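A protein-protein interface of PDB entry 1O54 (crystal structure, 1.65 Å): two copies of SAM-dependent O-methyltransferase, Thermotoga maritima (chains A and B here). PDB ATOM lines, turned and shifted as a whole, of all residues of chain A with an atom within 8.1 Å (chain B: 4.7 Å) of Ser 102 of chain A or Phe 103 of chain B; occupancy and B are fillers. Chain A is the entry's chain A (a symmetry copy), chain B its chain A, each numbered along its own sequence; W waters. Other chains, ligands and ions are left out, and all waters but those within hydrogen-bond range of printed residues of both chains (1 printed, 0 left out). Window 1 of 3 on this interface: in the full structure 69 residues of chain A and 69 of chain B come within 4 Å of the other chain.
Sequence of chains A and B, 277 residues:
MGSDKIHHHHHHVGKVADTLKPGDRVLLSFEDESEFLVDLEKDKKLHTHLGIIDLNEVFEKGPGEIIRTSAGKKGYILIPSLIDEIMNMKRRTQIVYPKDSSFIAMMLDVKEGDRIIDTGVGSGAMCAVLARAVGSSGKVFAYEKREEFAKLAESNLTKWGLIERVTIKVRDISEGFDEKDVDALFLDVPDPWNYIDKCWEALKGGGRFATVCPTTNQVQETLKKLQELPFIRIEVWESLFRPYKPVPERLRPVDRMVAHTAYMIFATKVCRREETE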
ATOM      1  N   ILE A  83      -6.524 -27.299  10.237  1.00  0.00           N
ATOM      2  CA  ILE A  83      -6.503 -27.840  11.619  1.00  0.00           C
ATOM      3  C   ILE A  83      -7.130 -29.213  11.684  1.00  0.00           C
ATOM      4  O   ILE A  83      -6.550 -30.183  12.247  1.00  0.00           O
ATOM      5  CB  ILE A  83      -7.216 -26.897  12.599  1.00  0.00           C
ATOM      6  CG1 ILE A  83      -6.370 -25.655  12.864  1.00  0.00           C
ATOM      7  CG2 ILE A  83      -7.480 -27.619  13.939  1.00  0.00           C
ATOM      8  CD1 ILE A  83      -7.044 -24.567  13.739  1.00  0.00           C
ATOM      9  N   VAL A  96       3.866 -30.352  15.499  1.00  0.00           N
ATOM     10  CA  VAL A  96       3.687 -29.059  16.157  1.00  0.00           C
ATOM     11  C   VAL A  96       2.191 -28.748  16.099  1.00  0.00           C
ATOM     12  O   VAL A  96       1.601 -28.716  14.996  1.00  0.00           O
ATOM     13  CB  VAL A  96       4.474 -27.928  15.474  1.00  0.00           C
ATOM     14  CG1 VAL A  96       4.247 -26.615  16.211  1.00  0.00           C
ATOM     15  CG2 VAL A  96       5.969 -28.246  15.437  1.00  0.00           C
ATOM     16  N   TYR A  97       1.567 -28.549  17.257  1.00  0.00           N
ATOM     17  CA  TYR A  97       0.115 -28.374  17.303  1.00  0.00           C
ATOM     18  C   TYR A  97      -0.237 -26.980  16.823  1.00  0.00           C
ATOM     19  O   TYR A  97       0.564 -26.052  16.997  1.00  0.00           O
ATOM     20  CB  TYR A  97      -0.438 -28.620  18.716  1.00  0.00           C
ATOM     21  CG  TYR A  97      -0.435 -30.103  19.039  1.00  0.00           C
ATOM     22  CD1 TYR A  97       0.714 -30.727  19.480  1.00  0.00           C
ATOM     23  CD2 TYR A  97      -1.590 -30.879  18.876  1.00  0.00           C
ATOM     24  CE1 TYR A  97       0.736 -32.101  19.754  1.00  0.00           C
ATOM     25  CE2 TYR A  97      -1.576 -32.254  19.151  1.00  0.00           C
ATOM     26  CZ  TYR A  97      -0.407 -32.850  19.590  1.00  0.00           C
ATOM     27  OH  TYR A  97      -0.383 -34.216  19.869  1.00  0.00           O
ATOM     28  N   PRO A  98      -1.417 -26.836  16.224  1.00  0.00           N
ATOM     29  CA  PRO A  98      -1.925 -25.541  15.765  1.00  0.00           C
ATOM     30  C   PRO A  98      -1.856 -24.370  16.728  1.00  0.00           C
ATOM     31  O   PRO A  98      -1.556 -23.257  16.300  1.00  0.00           O
ATOM     32  CB  PRO A  98      -3.405 -25.847  15.490  1.00  0.00           C
ATOM     33  CG  PRO A  98      -3.361 -27.250  14.987  1.00  0.00           C
ATOM     34  CD  PRO A  98      -2.361 -27.942  15.903  1.00  0.00           C
ATOM     35  N   LYS A  99      -2.149 -24.592  18.018  1.00  0.00           N
ATOM     36  CA  LYS A  99      -2.025 -23.503  18.998  1.00  0.00           C
ATOM     37  C   LYS A  99      -0.603 -22.928  18.982  1.00  0.00           C
ATOM     38  O   LYS A  99      -0.390 -21.737  19.201  1.00  0.00           O
ATOM     39  CB  LYS A  99      -2.370 -23.975  20.425  1.00  0.00           C
ATOM     40  CG  LYS A  99      -1.348 -24.915  21.104  1.00  0.00           C
ATOM     41  CD  LYS A  99      -1.637 -25.030  22.600  1.00  0.00           C
ATOM     42  CE  LYS A  99      -0.533 -25.617  23.375  1.00  0.00           C
ATOM     43  NZ  LYS A  99       0.570 -24.723  23.688  1.00  0.00           N
ATOM     44  N   ASP A 100       0.374 -23.774  18.688  1.00  0.00           N
ATOM     45  CA  ASP A 100       1.740 -23.300  18.631  1.00  0.00           C
ATOM     46  C   ASP A 100       2.089 -22.823  17.208  1.00  0.00           C
ATOM     47  O   ASP A 100       2.706 -21.802  17.063  1.00  0.00           O
ATOM     48  CB  ASP A 100       2.722 -24.389  19.070  1.00  0.00           C
ATOM     49  CG  ASP A 100       2.585 -24.772  20.546  1.00  0.00           C
ATOM     50  OD1 ASP A 100       2.188 -23.922  21.416  1.00  0.00           O
ATOM     51  OD2 ASP A 100       2.919 -25.922  20.925  1.00  0.00           O
ATOM     52  N   SER A 101       1.808 -23.630  16.187  1.00  0.00           N
ATOM     53  CA  SER A 101       2.231 -23.290  14.831  1.00  0.00           C
ATOM     54  C   SER A 101       1.732 -21.916  14.349  1.00  0.00           C
ATOM     55  O   SER A 101       2.489 -21.171  13.746  1.00  0.00           O
ATOM     56  CB  SER A 101       1.868 -24.411  13.838  1.00  0.00           C
ATOM     57  OG  SER A 101       0.497 -24.618  13.814  1.00  0.00           O
ATOM     58  N   SER A 102       0.479 -21.571  14.643  1.00  0.00           N
ATOM     59  CA  SER A 102      -0.075 -20.285  14.249  1.00  0.00           C
ATOM     60  C   SER A 102       0.719 -19.116  14.866  1.00  0.00           C
ATOM     61  O   SER A 102       1.095 -18.134  14.194  1.00  0.00           O
ATOM     62  CB  SER A 102      -1.571 -20.246  14.648  1.00  0.00           C
ATOM     63  OG  SER A 102      -1.801 -20.519  16.039  1.00  0.00           O
ATOM     64  N   PHE A 103       0.975 -19.247  16.160  1.00  0.00           N
ATOM     65  CA  PHE A 103       1.723 -18.257  16.899  1.00  0.00           C
ATOM     66  C   PHE A 103       3.158 -18.142  16.368  1.00  0.00           C
ATOM     67  O   PHE A 103       3.678 -17.024  16.149  1.00  0.00           O
ATOM     68  CB  PHE A 103       1.695 -18.628  18.372  1.00  0.00           C
ATOM     69  CG  PHE A 103       2.505 -17.701  19.249  1.00  0.00           C
ATOM     70  CD1 PHE A 103       2.075 -16.407  19.526  1.00  0.00           C
ATOM     71  CD2 PHE A 103       3.672 -18.152  19.836  1.00  0.00           C
ATOM     72  CE1 PHE A 103       2.830 -15.569  20.357  1.00  0.00           C
ATOM     73  CE2 PHE A 103       4.392 -17.351  20.670  1.00  0.00           C
ATOM     74  CZ  PHE A 103       3.975 -16.058  20.937  1.00  0.00           C
ATOM     75  N   ILE A 104       3.792 -19.290  16.161  1.00  0.00           N
ATOM     76  CA  ILE A 104       5.170 -19.288  15.677  1.00  0.00           C
ATOM     77  C   ILE A 104       5.260 -18.618  14.316  1.00  0.00           C
ATOM     78  O   ILE A 104       6.141 -17.796  14.088  1.00  0.00           O
ATOM     79  CB  ILE A 104       5.694 -20.705  15.603  1.00  0.00           C
ATOM     80  CG1 ILE A 104       5.888 -21.262  17.025  1.00  0.00           C
ATOM     81  CG2 ILE A 104       6.956 -20.745  14.786  1.00  0.00           C
ATOM     82  CD1 ILE A 104       6.057 -22.724  17.039  1.00  0.00           C
ATOM     83  N   ALA A 105       4.319 -18.906  13.422  1.00  0.00           N
ATOM     84  CA  ALA A 105       4.345 -18.309  12.075  1.00  0.00           C
ATOM     85  C   ALA A 105       4.169 -16.760  12.150  1.00  0.00           C
ATOM     86  O   ALA A 105       4.823 -16.013  11.420  1.00  0.00           O
ATOM     87  CB  ALA A 105       3.310 -18.960  11.176  1.00  0.00           C
ATOM     88  N   MET A 106       3.339 -16.270  13.064  1.00  0.00           N
ATOM     89  CA  MET A 106       3.178 -14.855  13.214  1.00  0.00           C
ATOM     90  C   MET A 106       4.407 -14.246  13.845  1.00  0.00           C
ATOM     91  O   MET A 106       4.829 -13.173  13.432  1.00  0.00           O
ATOM     92  CB  MET A 106       1.930 -14.496  14.000  1.00  0.00           C
ATOM     93  CG  MET A 106       1.564 -13.003  13.821  1.00  0.00           C
ATOM     94  SD  MET A 106       0.004 -12.606  14.582  1.00  0.00           S
ATOM     95  CE  MET A 106      -0.100 -10.777  14.260  1.00  0.00           C
ATOM     96  N   MET A 107       4.977 -14.909  14.849  1.00  0.00           N
ATOM     97  CA  MET A 107       6.208 -14.385  15.511  1.00  0.00           C
ATOM     98  C   MET A 107       7.391 -14.293  14.524  1.00  0.00           C
ATOM     99  O   MET A 107       8.202 -13.337  14.629  1.00  0.00           O
ATOM    100  CB  MET A 107       6.605 -15.215  16.724  1.00  0.00           C
ATOM    101  CG  MET A 107       5.612 -15.087  17.890  1.00  0.00           C
ATOM    102  SD  MET A 107       5.889 -13.591  18.826  1.00  0.00           S
ATOM    103  CE  MET A 107       7.256 -14.235  19.940  1.00  0.00           C
ATOM    104  N   LEU A 108       7.462 -15.272  13.608  1.00  0.00           N
ATOM    105  CA  LEU A 108       8.438 -15.285  12.487  1.00  0.00           C
ATOM    106  C   LEU A 108       8.112 -14.287  11.350  1.00  0.00           C
ATOM    107  O   LEU A 108       8.924 -14.106  10.413  1.00  0.00           O
ATOM    108  CB  LEU A 108       8.566 -16.690  11.914  1.00  0.00           C
ATOM    109  CG  LEU A 108       9.224 -17.738  12.804  1.00  0.00           C
ATOM    110  CD1 LEU A 108       9.285 -19.068  12.144  1.00  0.00           C
ATOM    111  CD2 LEU A 108      10.648 -17.307  13.229  1.00  0.00           C
ATOM    112  N   ASP A 109       6.972 -13.605  11.468  1.00  0.00           N
ATOM    113  CA  ASP A 109       6.532 -12.576  10.521  1.00  0.00           C
ATOM    114  C   ASP A 109       6.443 -13.119   9.097  1.00  0.00           C
ATOM    115  O   ASP A 109       6.704 -12.380   8.133  1.00  0.00           O
ATOM    116  CB  ASP A 109       7.448 -11.355  10.565  1.00  0.00           C
ATOM    117  CG  ASP A 109       6.798 -10.115   9.958  1.00  0.00           C
ATOM    118  OD1 ASP A 109       5.597  -9.833  10.217  1.00  0.00           O
ATOM    119  OD2 ASP A 109       7.460  -9.368   9.224  1.00  0.00           O
ATOM    120  N   VAL A 110       6.079 -14.398   8.961  1.00  0.00           N
ATOM    121  CA  VAL A 110       6.019 -15.031   7.641  1.00  0.00           C
ATOM    122  C   VAL A 110       4.932 -14.339   6.805  1.00  0.00           C
ATOM    123  O   VAL A 110       3.786 -14.200   7.237  1.00  0.00           O
ATOM    124  CB  VAL A 110       5.793 -16.555   7.691  1.00  0.00           C
ATOM    125  CG1 VAL A 110       5.850 -17.143   6.320  1.00  0.00           C
ATOM    126  CG2 VAL A 110       6.789 -17.230   8.636  1.00  0.00           C
ATOM    127  N   ALA A 125       2.914 -30.800   9.073  1.00  0.00           N
ATOM    128  CA  ALA A 125       1.879 -29.957   9.701  1.00  0.00           C
ATOM    129  C   ALA A 125       2.348 -28.502   9.848  1.00  0.00           C
ATOM    130  O   ALA A 125       1.669 -27.551   9.402  1.00  0.00           O
ATOM    131  CB  ALA A 125       1.447 -30.527  11.047  1.00  0.00           C
ATOM    132  N   MET A 126       3.512 -28.286  10.445  1.00  0.00           N
ATOM    133  CA  MET A 126       4.049 -26.928  10.576  1.00  0.00           C
ATOM    134  C   MET A 126       4.409 -26.363   9.191  1.00  0.00           C
ATOM    135  O   MET A 126       4.225 -25.184   8.915  1.00  0.00           O
ATOM    136  CB  MET A 126       5.263 -26.919  11.465  1.00  0.00           C
ATOM    137  CG  MET A 126       6.021 -25.655  11.512  1.00  0.00           C
ATOM    138  SD  MET A 126       4.964 -24.424  12.390  1.00  0.00           S
ATOM    139  CE  MET A 126       5.769 -22.976  12.191  1.00  0.00           C
ATOM    140  N   VAL A 129       1.521 -24.715   7.566  1.00  0.00           N
ATOM    141  CA  VAL A 129       1.220 -23.402   8.100  1.00  0.00           C
ATOM    142  C   VAL A 129       2.143 -22.342   7.462  1.00  0.00           C
ATOM    143  O   VAL A 129       1.713 -21.232   7.058  1.00  0.00           O
ATOM    144  CB  VAL A 129       1.360 -23.388   9.648  1.00  0.00           C
ATOM    145  CG1 VAL A 129       1.243 -21.999  10.202  1.00  0.00           C
ATOM    146  CG2 VAL A 129       0.300 -24.309  10.236  1.00  0.00           C
ATOM    147  N   LEU A 130       3.430 -22.672   7.385  1.00  0.00           N
ATOM    148  CA  LEU A 130       4.412 -21.784   6.784  1.00  0.00           C
ATOM    149  C   LEU A 130       4.084 -21.576   5.300  1.00  0.00           C
ATOM    150  O   LEU A 130       4.209 -20.458   4.800  1.00  0.00           O
ATOM    151  CB  LEU A 130       5.824 -22.389   6.956  1.00  0.00           C
ATOM    152  CG  LEU A 130       6.301 -22.500   8.427  1.00  0.00           C
ATOM    153  CD1 LEU A 130       7.616 -23.299   8.502  1.00  0.00           C
ATOM    154  CD2 LEU A 130       6.450 -21.133   9.096  1.00  0.00           C
ATOM    155  N   ALA A 133       1.394 -19.135   4.751  1.00  0.00           N
ATOM    156  CA  ALA A 133       1.846 -17.801   5.060  1.00  0.00           C
ATOM    157  C   ALA A 133       2.776 -17.144   4.032  1.00  0.00           C
ATOM    158  O   ALA A 133       2.815 -15.918   3.951  1.00  0.00           O
ATOM    159  CB  ALA A 133       2.512 -17.770   6.429  1.00  0.00           C
ATOM    160  N   PHE A 241      -3.894 -23.440  26.459  1.00  0.00           N
ATOM    161  CA  PHE A 241      -5.204 -23.176  25.872  1.00  0.00           C
ATOM    162  C   PHE A 241      -6.252 -23.982  26.611  1.00  0.00           C
ATOM    163  O   PHE A 241      -6.086 -25.181  26.826  1.00  0.00           O
ATOM    164  CB  PHE A 241      -5.221 -23.530  24.400  1.00  0.00           C
ATOM    165  CG  PHE A 241      -4.664 -22.480  23.510  1.00  0.00           C
ATOM    166  CD1 PHE A 241      -3.331 -22.121  23.585  1.00  0.00           C
ATOM    167  CD2 PHE A 241      -5.472 -21.828  22.606  1.00  0.00           C
ATOM    168  CE1 PHE A 241      -2.792 -21.169  22.754  1.00  0.00           C
ATOM    169  CE2 PHE A 241      -4.966 -20.879  21.765  1.00  0.00           C
ATOM    170  CZ  PHE A 241      -3.622 -20.515  21.845  1.00  0.00           C
ATOM    171  N   ARG A 242      -7.312 -23.309  27.030  1.00  0.00           N
ATOM    172  CA  ARG A 242      -8.343 -23.944  27.837  1.00  0.00           C
ATOM    173  C   ARG A 242      -9.675 -23.767  27.135  1.00  0.00           C
ATOM    174  O   ARG A 242     -10.094 -22.636  26.914  1.00  0.00           O
ATOM    175  CB  ARG A 242      -8.429 -23.272  29.220  1.00  0.00           C
ATOM    176  CG  ARG A 242      -9.413 -23.949  30.094  1.00  0.00           C
ATOM    177  CD  ARG A 242      -9.133 -23.813  31.604  1.00  0.00           C
ATOM    178  NE  ARG A 242      -9.345 -22.434  32.004  1.00  0.00           N
ATOM    179  CZ  ARG A 242      -9.378 -22.013  33.255  1.00  0.00           C
ATOM    180  NH1 ARG A 242      -9.235 -22.862  34.256  1.00  0.00           N
ATOM    181  NH2 ARG A 242      -9.578 -20.734  33.493  1.00  0.00           N
ATOM    182  N   MET A 264       8.621 -22.696  23.194  1.00  0.00           N
ATOM    183  CA  MET A 264       8.965 -22.045  21.948  1.00  0.00           C
ATOM    184  C   MET A 264      10.050 -21.011  22.180  1.00  0.00           C
ATOM    185  O   MET A 264       9.887 -20.139  23.048  1.00  0.00           O
ATOM    186  CB  MET A 264       7.742 -21.350  21.396  1.00  0.00           C
ATOM    187  CG  MET A 264       6.615 -22.313  21.124  1.00  0.00           C
ATOM    188  SD  MET A 264       5.039 -21.551  20.667  1.00  0.00           S
ATOM    189  CE  MET A 264       4.416 -20.982  22.294  1.00  0.00           C
ATOM    190  N   LYS B  99      -1.440 -13.065  20.078  1.00  0.00           N
ATOM    191  CA  LYS B  99      -1.642 -14.420  20.613  1.00  0.00           C
ATOM    192  C   LYS B  99      -3.046 -14.931  20.259  1.00  0.00           C
ATOM    193  O   LYS B  99      -3.258 -16.121  20.038  1.00  0.00           O
ATOM    194  CB  LYS B  99      -1.451 -14.467  22.142  1.00  0.00           C
ATOM    195  CG  LYS B  99      -2.553 -13.797  22.994  1.00  0.00           C
ATOM    196  CD  LYS B  99      -2.417 -14.201  24.461  1.00  0.00           C
ATOM    197  CE  LYS B  99      -3.604 -13.893  25.274  1.00  0.00           C
ATOM    198  NZ  LYS B  99      -4.716 -14.821  25.152  1.00  0.00           N
ATOM    199  N   ASP B 100      -4.002 -14.018  20.174  1.00  0.00           N
ATOM    200  CA  ASP B 100      -5.347 -14.420  19.823  1.00  0.00           C
ATOM    201  C   ASP B 100      -5.543 -14.379  18.295  1.00  0.00           C
ATOM    202  O   ASP B 100      -6.124 -15.279  17.750  1.00  0.00           O
ATOM    203  CB  ASP B 100      -6.388 -13.528  20.504  1.00  0.00           C
ATOM    204  CG  ASP B 100      -6.406 -13.672  22.028  1.00  0.00           C
ATOM    205  OD1 ASP B 100      -6.084 -14.774  22.593  1.00  0.00           O
ATOM    206  OD2 ASP B 100      -6.797 -12.714  22.740  1.00  0.00           O
ATOM    207  N   SER B 101      -5.176 -13.278  17.642  1.00  0.00           N
ATOM    208  CA  SER B 101      -5.455 -13.130  16.216  1.00  0.00           C
ATOM    209  C   SER B 101      -4.886 -14.267  15.349  1.00  0.00           C
ATOM    210  O   SER B 101      -5.565 -14.749  14.456  1.00  0.00           O
ATOM    211  CB  SER B 101      -5.013 -11.745  15.705  1.00  0.00           C
ATOM    212  OG  SER B 101      -3.651 -11.566  15.891  1.00  0.00           O
ATOM    213  N   SER B 102      -3.662 -14.713  15.633  1.00  0.00           N
ATOM    214  CA  SER B 102      -3.049 -15.798  14.882  1.00  0.00           C
ATOM    215  C   SER B 102      -3.880 -17.093  14.983  1.00  0.00           C
ATOM    216  O   SER B 102      -4.169 -17.782  13.983  1.00  0.00           O
ATOM    217  CB  SER B 102      -1.600 -15.997  15.392  1.00  0.00           C
ATOM    218  OG  SER B 102      -1.516 -16.217  16.809  1.00  0.00           O
ATOM    219  N   PHE B 103      -4.267 -17.406  16.211  1.00  0.00           N
ATOM    220  CA  PHE B 103      -5.068 -18.574  16.491  1.00  0.00           C
ATOM    221  C   PHE B 103      -6.440 -18.476  15.811  1.00  0.00           C
ATOM    222  O   PHE B 103      -6.916 -19.444  15.174  1.00  0.00           O
ATOM    223  CB  PHE B 103      -5.194 -18.726  17.997  1.00  0.00           C
ATOM    224  CG  PHE B 103      -6.071 -19.882  18.421  1.00  0.00           C
ATOM    225  CD1 PHE B 103      -5.649 -21.200  18.283  1.00  0.00           C
ATOM    226  CD2 PHE B 103      -7.299 -19.636  19.006  1.00  0.00           C
ATOM    227  CE1 PHE B 103      -6.469 -22.257  18.701  1.00  0.00           C
ATOM    228  CE2 PHE B 103      -8.086 -20.660  19.442  1.00  0.00           C
ATOM    229  CZ  PHE B 103      -7.674 -21.974  19.294  1.00  0.00           C
ATOM    230  N   ILE B 104      -7.070 -17.316  15.944  1.00  0.00           N
ATOM    231  CA  ILE B 104      -8.393 -17.129  15.352  1.00  0.00           C
ATOM    232  C   ILE B 104      -8.334 -17.294  13.843  1.00  0.00           C
ATOM    233  O   ILE B 104      -9.173 -17.975  13.262  1.00  0.00           O
ATOM    234  CB  ILE B 104      -8.931 -15.761  15.712  1.00  0.00           C
ATOM    235  CG1 ILE B 104      -9.276 -15.718  17.211  1.00  0.00           C
ATOM    236  CG2 ILE B 104     -10.105 -15.424  14.835  1.00  0.00           C
ATOM    237  CD1 ILE B 104      -9.472 -14.345  17.705  1.00  0.00           C
ATOM    238  N   ALA B 105      -7.312 -16.736  13.199  1.00  0.00           N
ATOM    239  CA  ALA B 105      -7.193 -16.840  11.734  1.00  0.00           C
ATOM    240  C   ALA B 105      -6.998 -18.325  11.296  1.00  0.00           C
ATOM    241  O   ALA B 105      -7.562 -18.767  10.294  1.00  0.00           O
ATOM    242  CB  ALA B 105      -6.084 -15.940  11.219  1.00  0.00           C
ATOM    243  N   MET B 106      -6.255 -19.111  12.067  1.00  0.00           N
ATOM    244  CA  MET B 106      -6.086 -20.496  11.743  1.00  0.00           C
ATOM    245  C   MET B 106      -7.360 -21.260  12.003  1.00  0.00           C
ATOM    246  O   MET B 106      -7.720 -22.122  11.210  1.00  0.00           O
ATOM    247  CB  MET B 106      -4.916 -21.122  12.481  1.00  0.00           C
ATOM    248  CG  MET B 106      -4.508 -22.472  11.843  1.00  0.00           C
ATOM    249  SD  MET B 106      -3.025 -23.131  12.576  1.00  0.00           S
ATOM    250  CE  MET B 106      -2.857 -24.743  11.664  1.00  0.00           C
ATOM    251  N   MET B 107      -8.040 -20.968  13.110  1.00  0.00           N
ATOM    252  CA  MET B 107      -9.322 -21.664  13.427  1.00  0.00           C
ATOM    253  C   MET B 107     -10.398 -21.395  12.354  1.00  0.00           C
ATOM    254  O   MET B 107     -11.199 -22.315  12.045  1.00  0.00           O
ATOM    255  CB  MET B 107      -9.853 -21.288  14.803  1.00  0.00           C
ATOM    256  CG  MET B 107      -8.981 -21.823  15.950  1.00  0.00           C
ATOM    257  SD  MET B 107      -9.324 -23.543  16.289  1.00  0.00           S
ATOM    258  CE  MET B 107     -10.806 -23.292  17.412  1.00  0.00           C
ATOM    259  N   TRP B 237     -12.789 -20.778  23.703  1.00  0.00           N
ATOM    260  CA  TRP B 237     -11.380 -20.940  24.074  1.00  0.00           C
ATOM    261  C   TRP B 237     -10.855 -19.690  24.780  1.00  0.00           C
ATOM    262  O   TRP B 237     -11.247 -18.557  24.462  1.00  0.00           O
ATOM    263  CB  TRP B 237     -10.526 -21.200  22.821  1.00  0.00           C
ATOM    264  CG  TRP B 237     -10.731 -22.539  22.265  1.00  0.00           C
ATOM    265  CD1 TRP B 237     -11.611 -22.916  21.268  1.00  0.00           C
ATOM    266  CD2 TRP B 237     -10.039 -23.730  22.653  1.00  0.00           C
ATOM    267  NE1 TRP B 237     -11.510 -24.278  21.044  1.00  0.00           N
ATOM    268  CE2 TRP B 237     -10.546 -24.790  21.870  1.00  0.00           C
ATOM    269  CE3 TRP B 237      -9.039 -24.013  23.586  1.00  0.00           C
ATOM    270  CZ2 TRP B 237     -10.077 -26.112  21.991  1.00  0.00           C
ATOM    271  CZ3 TRP B 237      -8.560 -25.316  23.694  1.00  0.00           C
ATOM    272  CH2 TRP B 237      -9.097 -26.349  22.932  1.00  0.00           C
ATOM    273  N   MET B 264     -12.640 -16.417  23.194  1.00  0.00           N
ATOM    274  CA  MET B 264     -12.846 -16.600  21.772  1.00  0.00           C
ATOM    275  C   MET B 264     -13.930 -17.632  21.529  1.00  0.00           C
ATOM    276  O   MET B 264     -13.840 -18.750  22.061  1.00  0.00           O
ATOM    277  CB  MET B 264     -11.562 -17.087  21.143  1.00  0.00           C
ATOM    278  CG  MET B 264     -10.430 -16.109  21.329  1.00  0.00           C
ATOM    279  SD  MET B 264      -8.803 -16.699  20.801  1.00  0.00           S
ATOM    280  CE  MET B 264      -8.337 -17.798  22.192  1.00  0.00           C
ATOM    281  N   PHE B 266     -16.195 -19.775  18.614  1.00  0.00           N
ATOM    282  CA  PHE B 266     -16.211 -20.220  17.223  1.00  0.00           C
ATOM    283  C   PHE B 266     -17.460 -21.027  16.955  1.00  0.00           C
ATOM    284  O   PHE B 266     -17.980 -21.685  17.848  1.00  0.00           O
ATOM    285  CB  PHE B 266     -14.993 -21.129  17.018  1.00  0.00           C
ATOM    286  CG  PHE B 266     -13.671 -20.449  17.294  1.00  0.00           C
ATOM    287  CD1 PHE B 266     -13.124 -20.496  18.561  1.00  0.00           C
ATOM    288  CD2 PHE B 266     -13.007 -19.760  16.325  1.00  0.00           C
ATOM    289  CE1 PHE B 266     -11.900 -19.842  18.850  1.00  0.00           C
ATOM    290  CE2 PHE B 266     -11.782 -19.126  16.598  1.00  0.00           C
ATOM    291  CZ  PHE B 266     -11.257 -19.166  17.872  1.00  0.00           C
HETATM  292  O   HOH W   1      -7.261 -24.425   9.711  1.00  0.00           O
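N of Trp 237 of chain B sits at hydrogen-bond distance from O of Met 264 of chain B (2.8 Å).
The side-chain hydroxyl (OG) of Ser 101 of chain A is in hydrogen-bond range of the backbone carbonyl oxygen (O) of Tyr 97 of chain A.
O of Pro 98 of chain A lies close to OG of Ser 101 of chain A (3.5 Å).
O of Pro 98 of chain A lies within hydrogen-bond range of OG of Ser 102 of chain A (2.8 Å).
Among the printed residues, pairs that only touch across the chains: Val 129 of chain A with Met 106 of chain B, Arg 242 of chain A with Trp 237 of chain B, Phe 241 of chain A with Phe 103 of chain B, Ile 83 of chain A with Met 107 of chain B, Ile 83 of chain A with Met 106 of chain B, Ser 102 of chain A with Ser 102 of chain B, Ser 102 of chain A with Phe 103 of chain B, Phe 103 of chain A with Ser 102 of chain B, Met 106 of chain A with Ser 102 of chain B, Ser 102 of chain A with Met 106 of chain B, Phe 241 of chain A with Trp 237 of chain B, Ser 101 of chain A with Met 106 of chain B and Met 106 of chain A with Ser 101 of chain B.
Ser 102 of chain A touches just these residues of chain B: Ser 102 (3.6 Å), Phe 103 (3.8 Å) and Met 106 (3.8 Å).
Of the printed residues of chain B, Met 106 of chain A touches Ser 101 and Ser 102.
Of the printed residues of chain A, Ser 101 of chain B touches Met 106 (3.99 Å).
Phe 103 of chain B touches just these residues of chain A: Ser 102 and Phe 241.
The nearest residue of chain A that does not touch Phe 103 of chain B is Lys 99 of chain A (4.4 Å).
Hydrophobic or aromatic side chains of chain A within 4 Å of the printed part of chain B: Ile 83, Met 106, Val 129 and Phe 241.
Of the 12 printed residues of chain B, 6 touch a printed residue of chain A.
Printed residues of chain B that touch a printed residue of chain A: Ser 101, Ser 102, Phe 103, Met 106, Met 107 and Trp 237.
Hydrophobic or aromatic side chains of chain B within 4 Å of the printed part of chain A: Phe 103, Met 106, Met 107 and Trp 237.
Ser 101 of chain A touches Met 106 of chain B, and with the chains exchanged Met 106 of chain A touches Ser 101 of chain B.
Ser 102 of chain B touches its own counterpart, Ser 102 of chain A.
Ser 102 of chain A touches Phe 103 of chain B, and with the chains exchanged Phe 103 of chain A touches Ser 102 of chain B.
Ser 102 of chain A touches Met 106 of chain B, and with the chains exchanged Met 106 of chain A touches Ser 102 of chain B.
10 positions are printed for both chains.
Of the 13 pairs that touch across the chains among the printed residues, 7 have their exchanged pair printed and touching as well.
Water W1 lies within hydrogen-bond range of O of Met 106 of chain B (2.8 Å) and N of Ile 83 of chain A (3.0 Å).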
